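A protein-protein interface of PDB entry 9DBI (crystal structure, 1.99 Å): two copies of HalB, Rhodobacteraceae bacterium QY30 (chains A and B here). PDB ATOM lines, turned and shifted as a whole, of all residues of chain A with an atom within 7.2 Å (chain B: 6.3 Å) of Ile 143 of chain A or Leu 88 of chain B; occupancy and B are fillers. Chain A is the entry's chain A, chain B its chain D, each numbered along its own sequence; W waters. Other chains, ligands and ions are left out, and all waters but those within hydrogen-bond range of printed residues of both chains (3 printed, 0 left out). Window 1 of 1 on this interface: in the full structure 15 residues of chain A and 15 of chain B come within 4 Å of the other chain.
O of Phe 69 of chain A sits at hydrogen-bond distance from NZ of Lys 85 of chain B, at 2.7 Å. The backbone NH (N) of Ile 90 of chain B sits at hydrogen-bond distance from the backbone carbonyl oxygen (O) of Gly 141 of chain A (2.6 Å). The backbone carbonyl oxygen (O) of Glu 86 of chain B sits at hydrogen-bond distance from the side-chain amino group (NZ) of Lys 142 of chain A (2.9 Å). The side-chain amino group of Lys 142 of chain A sits at hydrogen-bond distance from the backbone carbonyl oxygen of Leu 88 of chain B (3.0 Å). The backbone carbonyl oxygen (O) of Phe 69 of chain A sits close to the backbone carbonyl oxygen (O) of Ala 68 of chain B.
The side-chain hydroxyl of Ser 140 of chain A sits at hydrogen-bond distance from the backbone carbonyl oxygen of Leu 137 of chain A (2.8 Å). The backbone carbonyl oxygen of Leu 137 of chain A sits at hydrogen-bond distance from the backbone NH of Lys 142 of chain A (3.0 Å). The backbone carbonyl oxygen (O) of Ala 57 of chain B lies within hydrogen-bond range of the backbone NH (N) of Val 89 of chain B, at 3.1 Å.
Among the printed residues, pairs that only touch across the chains: Gly 141 of chain A with Val 89 of chain B (3.4 Å), Ile 143 of chain A with Lys 85 of chain B (3.5 Å), Lys 142 of chain A with Arg 87 of chain B (3.5 Å), Lys 142 of chain A with Val 89 of chain B (3.6 Å), Ile 144 of chain A with Glu 86 of chain B (3.6 Å), Ser 140 of chain A with Val 89 of chain B (3.8 Å), Gly 141 of chain A with Leu 88 of chain B (3.8 Å) and Ile 143 of chain A with Leu 88 of chain B (3.8 Å).
Printed residues of chain B within 4 Å of Phe 69 of chain A: Ala 68 (3.4 Å) and Lys 85 (2.7 Å). Ile 90 of chain A touches none of the printed residues of chain B. Ile 143 of chain A touches just these residues of chain B: Lys 85 and Leu 88. Of the printed residues of chain A, Lys 85 of chain B touches Phe 69 (2.7 Å) and Ile 143 (3.5 Å). Of the printed residues of chain A, Leu 88 of chain B touches Gly 141, Lys 142 and Ile 143. The nearest residue of chain B that does not touch Ile 143 of chain A is Ala 68 of chain B (4.2 Å). The nearest residue of chain A that does not touch Leu 88 of chain B is Phe 69 of chain A (4.2 Å).
Along chain A the printed residues that touch a printed residue of chain B span positions 69 to 144. Hydrophobic or aromatic side chains of chain B within 4 Å of the printed part of chain A: Ala 68, Leu 88, Val 89 and Ile 90. Among the printed residues, 13 pairs touch across the chains.
2 positions are printed for both chains.
Water W1 lies within hydrogen-bond range of the backbone carbonyl oxygen (O) of Leu 88 of chain B (2.7 Å), the backbone NH (N) of Ile 143 of chain A (2.7 Å) and the backbone carbonyl oxygen (O) of Lys 85 of chain B (2.8 Å). Water W3 lies within hydrogen-bond range of O of Ala 68 of chain B and O of Phe 69 of chain A. Water W2 bridges the side-chain amino group (NZ) of Lys 85 of chain B (3.2 Å) and the backbone carbonyl oxygen (O) of Phe 69 of chain A (3.4 Å).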
ATOM      1  N   ILE A  65       6.919  -7.011   6.646  1.00  0.00           N
ATOM      2  CA  ILE A  65       6.755  -8.195   7.488  1.00  0.00           C
ATOM      3  C   ILE A  65       5.619  -9.054   6.958  1.00  0.00           C
ATOM      4  O   ILE A  65       5.738 -10.282   6.870  1.00  0.00           O
ATOM      5  CB  ILE A  65       6.509  -7.797   8.958  1.00  0.00           C
ATOM      6  CG1 ILE A  65       7.696  -7.004   9.503  1.00  0.00           C
ATOM      7  CG2 ILE A  65       6.231  -9.065   9.829  1.00  0.00           C
ATOM      8  CD1 ILE A  65       7.503  -6.440  10.917  1.00  0.00           C
ATOM      9  N   HIS A  66       4.492  -8.419   6.616  1.00  0.00           N
ATOM     10  CA  HIS A  66       3.392  -9.159   6.021  1.00  0.00           C
ATOM     11  C   HIS A  66       3.836  -9.887   4.755  1.00  0.00           C
ATOM     12  O   HIS A  66       3.535 -11.072   4.580  1.00  0.00           O
ATOM     13  CB  HIS A  66       2.229  -8.223   5.712  1.00  0.00           C
ATOM     14  CG  HIS A  66       1.243  -8.812   4.749  1.00  0.00           C
ATOM     15  ND1 HIS A  66       0.391  -9.842   5.090  1.00  0.00           N
ATOM     16  CD2 HIS A  66       0.999  -8.537   3.445  1.00  0.00           C
ATOM     17  CE1 HIS A  66      -0.341 -10.170   4.040  1.00  0.00           C
ATOM     18  NE2 HIS A  66       0.007  -9.392   3.031  1.00  0.00           N
ATOM     19  N   PHE A  69       6.068 -13.009   5.657  1.00  0.00           N
ATOM     20  CA  PHE A  69       5.508 -14.110   6.422  1.00  0.00           C
ATOM     21  C   PHE A  69       4.198 -14.654   5.863  1.00  0.00           C
ATOM     22  O   PHE A  69       3.816 -15.778   6.221  1.00  0.00           O
ATOM     23  CB  PHE A  69       5.315 -13.687   7.890  1.00  0.00           C
ATOM     24  CG  PHE A  69       6.580 -13.814   8.729  1.00  0.00           C
ATOM     25  CD1 PHE A  69       6.986 -15.058   9.222  1.00  0.00           C
ATOM     26  CD2 PHE A  69       7.372 -12.702   9.014  1.00  0.00           C
ATOM     27  CE1 PHE A  69       8.168 -15.190   9.994  1.00  0.00           C
ATOM     28  CE2 PHE A  69       8.539 -12.818   9.808  1.00  0.00           C
ATOM     29  CZ  PHE A  69       8.927 -14.067  10.310  1.00  0.00           C
ATOM     30  N   GLU A  70       3.520 -13.906   4.987  1.00  0.00           N
ATOM     31  CA  GLU A  70       2.243 -14.331   4.422  1.00  0.00           C
ATOM     32  C   GLU A  70       2.172 -14.275   2.909  1.00  0.00           C
ATOM     33  O   GLU A  70       1.254 -14.878   2.340  1.00  0.00           O
ATOM     34  CB  GLU A  70       1.091 -13.487   4.988  1.00  0.00           C
ATOM     35  CG  GLU A  70       0.965 -13.617   6.500  1.00  0.00           C
ATOM     36  CD  GLU A  70      -0.301 -12.995   7.052  1.00  0.00           C
ATOM     37  OE1 GLU A  70      -0.652 -11.871   6.634  1.00  0.00           O
ATOM     38  OE2 GLU A  70      -0.950 -13.644   7.902  1.00  0.00           O
ATOM     39  N   ILE A  90      13.286  -6.919  11.679  1.00  0.00           N
ATOM     40  CA  ILE A  90      12.103  -6.680  12.507  1.00  0.00           C
ATOM     41  C   ILE A  90      12.526  -5.887  13.736  1.00  0.00           C
ATOM     42  O   ILE A  90      13.358  -6.347  14.529  1.00  0.00           O
ATOM     43  CB  ILE A  90      11.440  -8.002  12.915  1.00  0.00           C
ATOM     44  CG1 ILE A  90      11.024  -8.797  11.680  1.00  0.00           C
ATOM     45  CG2 ILE A  90      10.235  -7.749  13.833  1.00  0.00           C
ATOM     46  CD1 ILE A  90      10.478 -10.184  12.011  1.00  0.00           C
ATOM     47  N   ILE A 134      -1.481  -4.337  14.957  1.00  0.00           N
ATOM     48  CA  ILE A 134      -0.410  -5.088  14.299  1.00  0.00           C
ATOM     49  C   ILE A 134       0.935  -4.741  14.926  1.00  0.00           C
ATOM     50  O   ILE A 134       1.739  -5.625  15.256  1.00  0.00           O
ATOM     51  CB  ILE A 134      -0.415  -4.813  12.784  1.00  0.00           C
ATOM     52  CG1 ILE A 134      -1.641  -5.450  12.126  1.00  0.00           C
ATOM     53  CG2 ILE A 134       0.864  -5.345  12.115  1.00  0.00           C
ATOM     54  CD1 ILE A 134      -1.910  -4.934  10.694  1.00  0.00           C
ATOM     55  N   LEU A 137       1.466  -6.173  18.341  1.00  0.00           N
ATOM     56  CA  LEU A 137       1.682  -7.616  18.310  1.00  0.00           C
ATOM     57  C   LEU A 137       3.076  -7.946  17.788  1.00  0.00           C
ATOM     58  O   LEU A 137       3.742  -8.840  18.326  1.00  0.00           O
ATOM     59  CB  LEU A 137       0.591  -8.307  17.484  1.00  0.00           C
ATOM     60  CG  LEU A 137      -0.767  -8.310  18.206  1.00  0.00           C
ATOM     61  CD1 LEU A 137      -1.898  -8.720  17.277  1.00  0.00           C
ATOM     62  CD2 LEU A 137      -0.750  -9.190  19.470  1.00  0.00           C
ATOM     63  N   VAL A 138       3.557  -7.203  16.783  1.00  0.00           N
ATOM     64  CA  VAL A 138       4.926  -7.417  16.303  1.00  0.00           C
ATOM     65  C   VAL A 138       5.927  -7.141  17.417  1.00  0.00           C
ATOM     66  O   VAL A 138       6.893  -7.897  17.602  1.00  0.00           O
ATOM     67  CB  VAL A 138       5.210  -6.562  15.055  1.00  0.00           C
ATOM     68  CG1 VAL A 138       6.722  -6.477  14.795  1.00  0.00           C
ATOM     69  CG2 VAL A 138       4.489  -7.137  13.854  1.00  0.00           C
ATOM     70  N   SER A 140       5.516  -7.723  20.416  1.00  0.00           N
ATOM     71  CA  SER A 140       5.514  -8.874  21.304  1.00  0.00           C
ATOM     72  C   SER A 140       5.967 -10.141  20.600  1.00  0.00           C
ATOM     73  O   SER A 140       5.953 -11.207  21.218  1.00  0.00           O
ATOM     74  CB  SER A 140       4.129  -9.088  21.908  1.00  0.00           C
ATOM     75  OG  SER A 140       3.273  -9.629  20.923  1.00  0.00           O
ATOM     76  N   GLY A 141       6.379 -10.047  19.341  1.00  0.00           N
ATOM     77  CA  GLY A 141       6.958 -11.165  18.635  1.00  0.00           C
ATOM     78  C   GLY A 141       6.013 -11.968  17.763  1.00  0.00           C
ATOM     79  O   GLY A 141       6.370 -13.086  17.372  1.00  0.00           O
ATOM     80  N   LYS A 142       4.834 -11.438  17.443  1.00  0.00           N
ATOM     81  CA  LYS A 142       3.830 -12.150  16.669  1.00  0.00           C
ATOM     82  C   LYS A 142       3.739 -11.575  15.262  1.00  0.00           C
ATOM     83  O   LYS A 142       4.206 -10.468  14.982  1.00  0.00           O
ATOM     84  CB  LYS A 142       2.474 -12.109  17.382  1.00  0.00           C
ATOM     85  CG  LYS A 142       2.587 -12.691  18.792  1.00  0.00           C
ATOM     86  CD  LYS A 142       1.254 -13.045  19.405  1.00  0.00           C
ATOM     87  CE  LYS A 142       0.537 -14.124  18.599  1.00  0.00           C
ATOM     88  NZ  LYS A 142       1.173 -15.455  18.693  1.00  0.00           N
ATOM     89  N   ILE A 143       3.171 -12.370  14.363  1.00  0.00           N
ATOM     90  CA  ILE A 143       3.090 -12.019  12.953  1.00  0.00           C
ATOM     91  C   ILE A 143       1.625 -12.054  12.538  1.00  0.00           C
ATOM     92  O   ILE A 143       1.234 -12.830  11.664  1.00  0.00           O
ATOM     93  CB  ILE A 143       3.960 -12.953  12.070  1.00  0.00           C
ATOM     94  CG1 ILE A 143       3.599 -14.449  12.241  1.00  0.00           C
ATOM     95  CG2 ILE A 143       5.421 -12.776  12.391  1.00  0.00           C
ATOM     96  CD1 ILE A 143       4.127 -15.406  11.115  1.00  0.00           C
ATOM     97  N   ILE A 144       0.809 -11.179  13.115  1.00  0.00           N
ATOM     98  CA  ILE A 144      -0.633 -11.201  12.896  1.00  0.00           C
ATOM     99  C   ILE A 144      -1.027 -10.058  11.973  1.00  0.00           C
ATOM    100  O   ILE A 144      -0.656  -8.906  12.212  1.00  0.00           O
ATOM    101  CB  ILE A 144      -1.404 -11.112  14.221  1.00  0.00           C
ATOM    102  CG1 ILE A 144      -0.895 -12.168  15.200  1.00  0.00           C
ATOM    103  CG2 ILE A 144      -2.891 -11.277  13.965  1.00  0.00           C
ATOM    104  CD1 ILE A 144      -1.328 -13.565  14.873  1.00  0.00           C
ATOM    105  N   PHE A 145      -1.807 -10.372  10.932  1.00  0.00           N
ATOM    106  CA  PHE A 145      -2.340  -9.318  10.073  1.00  0.00           C
ATOM    107  C   PHE A 145      -3.820  -9.468   9.751  1.00  0.00           C
ATOM    108  O   PHE A 145      -4.462  -8.454   9.471  1.00  0.00           O
ATOM    109  CB  PHE A 145      -1.535  -9.245   8.763  1.00  0.00           C
ATOM    110  CG  PHE A 145      -0.090  -8.892   8.973  1.00  0.00           C
ATOM    111  CD1 PHE A 145       0.842  -9.883   9.217  1.00  0.00           C
ATOM    112  CD2 PHE A 145       0.330  -7.562   8.952  1.00  0.00           C
ATOM    113  CE1 PHE A 145       2.178  -9.559   9.435  1.00  0.00           C
ATOM    114  CE2 PHE A 145       1.663  -7.237   9.164  1.00  0.00           C
ATOM    115  CZ  PHE A 145       2.575  -8.230   9.414  1.00  0.00           C
ATOM    116  N   SER A 146      -4.362 -10.678   9.743  1.00  0.00           N
ATOM    117  CA  SER A 146      -5.770 -10.936   9.498  1.00  0.00           C
ATOM    118  C   SER A 146      -6.640 -10.153  10.482  1.00  0.00           C
ATOM    119  O   SER A 146      -6.441 -10.275  11.696  1.00  0.00           O
ATOM    120  CB  SER A 146      -6.024 -12.433   9.632  1.00  0.00           C
ATOM    121  OG  SER A 146      -7.404 -12.702   9.692  1.00  0.00           O
ATOM    122  N   LEU A 150      -6.530 -10.284  14.559  1.00  0.00           N
ATOM    123  CA  LEU A 150      -6.189  -9.060  15.296  1.00  0.00           C
ATOM    124  C   LEU A 150      -7.162  -8.800  16.432  1.00  0.00           C
ATOM    125  O   LEU A 150      -6.758  -8.428  17.541  1.00  0.00           O
ATOM    126  CB  LEU A 150      -6.190  -7.850  14.349  1.00  0.00           C
ATOM    127  CG  LEU A 150      -5.026  -7.728  13.368  1.00  0.00           C
ATOM    128  CD1 LEU A 150      -5.169  -6.520  12.419  1.00  0.00           C
ATOM    129  CD2 LEU A 150      -3.746  -7.646  14.158  1.00  0.00           C
ATOM    130  N   LEU B  54       1.812 -26.542  16.172  1.00  0.00           N
ATOM    131  CA  LEU B  54       1.399 -25.320  16.859  1.00  0.00           C
ATOM    132  C   LEU B  54       2.258 -25.065  18.088  1.00  0.00           C
ATOM    133  O   LEU B  54       2.569 -23.912  18.409  1.00  0.00           O
ATOM    134  CB  LEU B  54      -0.083 -25.380  17.265  1.00  0.00           C
ATOM    135  CG  LEU B  54      -1.193 -25.549  16.202  1.00  0.00           C
ATOM    136  CD1 LEU B  54      -2.530 -24.884  16.567  1.00  0.00           C
ATOM    137  CD2 LEU B  54      -0.751 -25.106  14.838  1.00  0.00           C
ATOM    138  N   SER B  56       5.433 -25.826  18.470  1.00  0.00           N
ATOM    139  CA  SER B  56       6.746 -25.297  18.114  1.00  0.00           C
ATOM    140  C   SER B  56       6.668 -23.805  17.808  1.00  0.00           C
ATOM    141  O   SER B  56       7.597 -23.060  18.138  1.00  0.00           O
ATOM    142  CB  SER B  56       7.341 -26.061  16.932  1.00  0.00           C
ATOM    143  OG  SER B  56       6.670 -25.708  15.746  1.00  0.00           O
ATOM    144  N   ALA B  57       5.546 -23.351  17.231  1.00  0.00           N
ATOM    145  CA  ALA B  57       5.322 -21.925  17.008  1.00  0.00           C
ATOM    146  C   ALA B  57       5.210 -21.161  18.324  1.00  0.00           C
ATOM    147  O   ALA B  57       5.844 -20.111  18.492  1.00  0.00           O
ATOM    148  CB  ALA B  57       4.072 -21.715  16.144  1.00  0.00           C
ATOM    149  N   SER B  58       4.408 -21.669  19.273  1.00  0.00           N
ATOM    150  CA  SER B  58       4.284 -21.002  20.566  1.00  0.00           C
ATOM    151  C   SER B  58       5.617 -20.949  21.285  1.00  0.00           C
ATOM    152  O   SER B  58       5.885 -20.010  22.045  1.00  0.00           O
ATOM    153  CB  SER B  58       3.270 -21.713  21.472  1.00  0.00           C
ATOM    154  OG  SER B  58       2.061 -21.988  20.805  1.00  0.00           O
ATOM    155  N   GLY B  60       8.406 -20.579  19.839  1.00  0.00           N
ATOM    156  CA  GLY B  60       9.350 -19.823  19.036  1.00  0.00           C
ATOM    157  C   GLY B  60      10.544 -20.603  18.521  1.00  0.00           C
ATOM    158  O   GLY B  60      11.603 -20.009  18.309  1.00  0.00           O
ATOM    159  N   ASP B  61      10.410 -21.917  18.315  1.00  0.00           N
ATOM    160  CA  ASP B  61      11.526 -22.701  17.790  1.00  0.00           C
ATOM    161  C   ASP B  61      12.035 -22.122  16.472  1.00  0.00           C
ATOM    162  O   ASP B  61      11.249 -21.669  15.634  1.00  0.00           O
ATOM    163  CB  ASP B  61      11.109 -24.155  17.558  1.00  0.00           C
ATOM    164  CG  ASP B  61      10.731 -24.887  18.840  1.00  0.00           C
ATOM    165  OD1 ASP B  61      11.232 -24.528  19.929  1.00  0.00           O
ATOM    166  OD2 ASP B  61       9.933 -25.833  18.744  1.00  0.00           O
ATOM    167  N   ALA B  64      10.313 -23.535  13.523  1.00  0.00           N
ATOM    168  CA  ALA B  64       9.010 -22.943  13.242  1.00  0.00           C
ATOM    169  C   ALA B  64       9.155 -21.583  12.569  1.00  0.00           C
ATOM    170  O   ALA B  64       8.385 -21.255  11.656  1.00  0.00           O
ATOM    171  CB  ALA B  64       8.186 -22.831  14.529  1.00  0.00           C
ATOM    172  N   ILE B  65      10.147 -20.784  12.991  1.00  0.00           N
ATOM    173  CA  ILE B  65      10.389 -19.510  12.324  1.00  0.00           C
ATOM    174  C   ILE B  65      10.694 -19.737  10.849  1.00  0.00           C
ATOM    175  O   ILE B  65      10.139 -19.053   9.979  1.00  0.00           O
ATOM    176  CB  ILE B  65      11.511 -18.719  13.021  1.00  0.00           C
ATOM    177  CG1 ILE B  65      11.131 -18.368  14.462  1.00  0.00           C
ATOM    178  CG2 ILE B  65      11.800 -17.427  12.271  1.00  0.00           C
ATOM    179  CD1 ILE B  65      12.257 -17.613  15.241  1.00  0.00           C
ATOM    180  N   ALA B  68       7.544 -20.612   8.844  1.00  0.00           N
ATOM    181  CA  ALA B  68       6.647 -19.480   8.644  1.00  0.00           C
ATOM    182  C   ALA B  68       7.197 -18.478   7.633  1.00  0.00           C
ATOM    183  O   ALA B  68       6.425 -17.853   6.887  1.00  0.00           O
ATOM    184  CB  ALA B  68       6.390 -18.789   9.981  1.00  0.00           C
ATOM    185  N   ARG B  83      -3.299 -21.375  11.527  1.00  0.00           N
ATOM    186  CA  ARG B  83      -3.254 -21.421  12.984  1.00  0.00           C
ATOM    187  C   ARG B  83      -1.824 -21.528  13.487  1.00  0.00           C
ATOM    188  O   ARG B  83      -1.491 -20.999  14.554  1.00  0.00           O
ATOM    189  CB  ARG B  83      -4.083 -22.600  13.495  1.00  0.00           C
ATOM    190  CG  ARG B  83      -5.582 -22.356  13.417  1.00  0.00           C
ATOM    191  CD  ARG B  83      -6.339 -23.573  13.931  1.00  0.00           C
ATOM    192  NE  ARG B  83      -6.594 -24.517  12.850  1.00  0.00           N
ATOM    193  CZ  ARG B  83      -6.164 -25.771  12.810  1.00  0.00           C
ATOM    194  NH1 ARG B  83      -5.465 -26.303  13.807  1.00  0.00           N
ATOM    195  NH2 ARG B  83      -6.454 -26.519  11.747  1.00  0.00           N
ATOM    196  N   PHE B  84      -0.968 -22.207  12.731  1.00  0.00           N
ATOM    197  CA  PHE B  84       0.444 -22.260  13.074  1.00  0.00           C
ATOM    198  C   PHE B  84       1.047 -20.858  13.107  1.00  0.00           C
ATOM    199  O   PHE B  84       1.693 -20.476  14.082  1.00  0.00           O
ATOM    200  CB  PHE B  84       1.150 -23.173  12.077  1.00  0.00           C
ATOM    201  CG  PHE B  84       2.639 -23.023  12.036  1.00  0.00           C
ATOM    202  CD1 PHE B  84       3.434 -23.499  13.074  1.00  0.00           C
ATOM    203  CD2 PHE B  84       3.250 -22.463  10.925  1.00  0.00           C
ATOM    204  CE1 PHE B  84       4.827 -23.384  13.016  1.00  0.00           C
ATOM    205  CE2 PHE B  84       4.643 -22.343  10.851  1.00  0.00           C
ATOM    206  CZ  PHE B  84       5.430 -22.801  11.904  1.00  0.00           C
ATOM    207  N   LYS B  85       0.810 -20.058  12.069  1.00  0.00           N
ATOM    208  CA  LYS B  85       1.440 -18.741  12.016  1.00  0.00           C
ATOM    209  C   LYS B  85       0.852 -17.796  13.057  1.00  0.00           C
ATOM    210  O   LYS B  85       1.570 -16.951  13.605  1.00  0.00           O
ATOM    211  CB  LYS B  85       1.306 -18.155  10.608  1.00  0.00           C
ATOM    212  CG  LYS B  85       2.113 -18.932   9.567  1.00  0.00           C
ATOM    213  CD  LYS B  85       2.073 -18.263   8.179  1.00  0.00           C
ATOM    214  CE  LYS B  85       2.976 -19.003   7.194  1.00  0.00           C
ATOM    215  NZ  LYS B  85       3.057 -18.338   5.869  1.00  0.00           N
ATOM    216  N   GLU B  86      -0.438 -17.935  13.361  1.00  0.00           N
ATOM    217  CA  GLU B  86      -1.032 -17.159  14.437  1.00  0.00           C
ATOM    218  C   GLU B  86      -0.485 -17.540  15.806  1.00  0.00           C
ATOM    219  O   GLU B  86      -0.545 -16.723  16.723  1.00  0.00           O
ATOM    220  CB  GLU B  86      -2.546 -17.320  14.411  1.00  0.00           C
ATOM    221  CG  GLU B  86      -3.146 -16.723  13.167  1.00  0.00           C
ATOM    222  CD  GLU B  86      -4.649 -16.850  13.136  1.00  0.00           C
ATOM    223  OE1 GLU B  86      -5.218 -17.414  14.097  1.00  0.00           O
ATOM    224  OE2 GLU B  86      -5.251 -16.383  12.146  1.00  0.00           O
ATOM    225  N   ARG B  87       0.047 -18.752  15.975  1.00  0.00           N
ATOM    226  CA  ARG B  87       0.610 -19.129  17.263  1.00  0.00           C
ATOM    227  C   ARG B  87       2.070 -18.715  17.426  1.00  0.00           C
ATOM    228  O   ARG B  87       2.567 -18.697  18.557  1.00  0.00           O
ATOM    229  CB  ARG B  87       0.485 -20.642  17.487  1.00  0.00           C
ATOM    230  CG  ARG B  87      -0.951 -21.149  17.622  1.00  0.00           C
ATOM    231  CD  ARG B  87      -1.554 -21.019  19.026  1.00  0.00           C
ATOM    232  NE  ARG B  87      -1.442 -19.687  19.616  1.00  0.00           N
ATOM    233  CZ  ARG B  87      -2.231 -18.650  19.352  1.00  0.00           C
ATOM    234  NH1 ARG B  87      -3.208 -18.723  18.458  1.00  0.00           N
ATOM    235  NH2 ARG B  87      -2.029 -17.505  20.000  1.00  0.00           N
ATOM    236  N   LEU B  88       2.759 -18.380  16.338  1.00  0.00           N
ATOM    237  CA  LEU B  88       4.182 -18.068  16.419  1.00  0.00           C
ATOM    238  C   LEU B  88       4.423 -16.899  17.356  1.00  0.00           C
ATOM    239  O   LEU B  88       3.761 -15.857  17.256  1.00  0.00           O
ATOM    240  CB  LEU B  88       4.740 -17.732  15.033  1.00  0.00           C
ATOM    241  CG  LEU B  88       6.257 -17.511  14.927  1.00  0.00           C
ATOM    242  CD1 LEU B  88       6.983 -18.790  15.262  1.00  0.00           C
ATOM    243  CD2 LEU B  88       6.707 -16.956  13.508  1.00  0.00           C
ATOM    244  N   VAL B  89       5.360 -17.080  18.285  1.00  0.00           N
ATOM    245  CA  VAL B  89       5.898 -15.998  19.099  1.00  0.00           C
ATOM    246  C   VAL B  89       7.405 -16.037  18.906  1.00  0.00           C
ATOM    247  O   VAL B  89       8.066 -16.989  19.335  1.00  0.00           O
ATOM    248  CB  VAL B  89       5.529 -16.129  20.584  1.00  0.00           C
ATOM    249  CG1 VAL B  89       6.168 -14.987  21.381  1.00  0.00           C
ATOM    250  CG2 VAL B  89       3.994 -16.138  20.770  1.00  0.00           C
ATOM    251  N   ILE B  90       7.951 -15.023  18.248  1.00  0.00           N
ATOM    252  CA  ILE B  90       9.394 -14.943  18.044  1.00  0.00           C
ATOM    253  C   ILE B  90      10.033 -14.394  19.314  1.00  0.00           C
ATOM    254  O   ILE B  90       9.667 -13.314  19.782  1.00  0.00           O
ATOM    255  CB  ILE B  90       9.735 -14.062  16.837  1.00  0.00           C
ATOM    256  CG1 ILE B  90       9.212 -14.687  15.537  1.00  0.00           C
ATOM    257  CG2 ILE B  90      11.248 -13.820  16.774  1.00  0.00           C
ATOM    258  CD1 ILE B  90       9.301 -13.722  14.320  1.00  0.00           C
HETATM  259  O   HOH W   1       2.229 -14.786  15.265  1.00  0.00           O
HETATM  260  O   HOH W   2       3.968 -17.008   3.091  1.00  0.00           O
HETATM  261  O   HOH W   3       6.396 -16.910   4.297  1.00  0.00           O
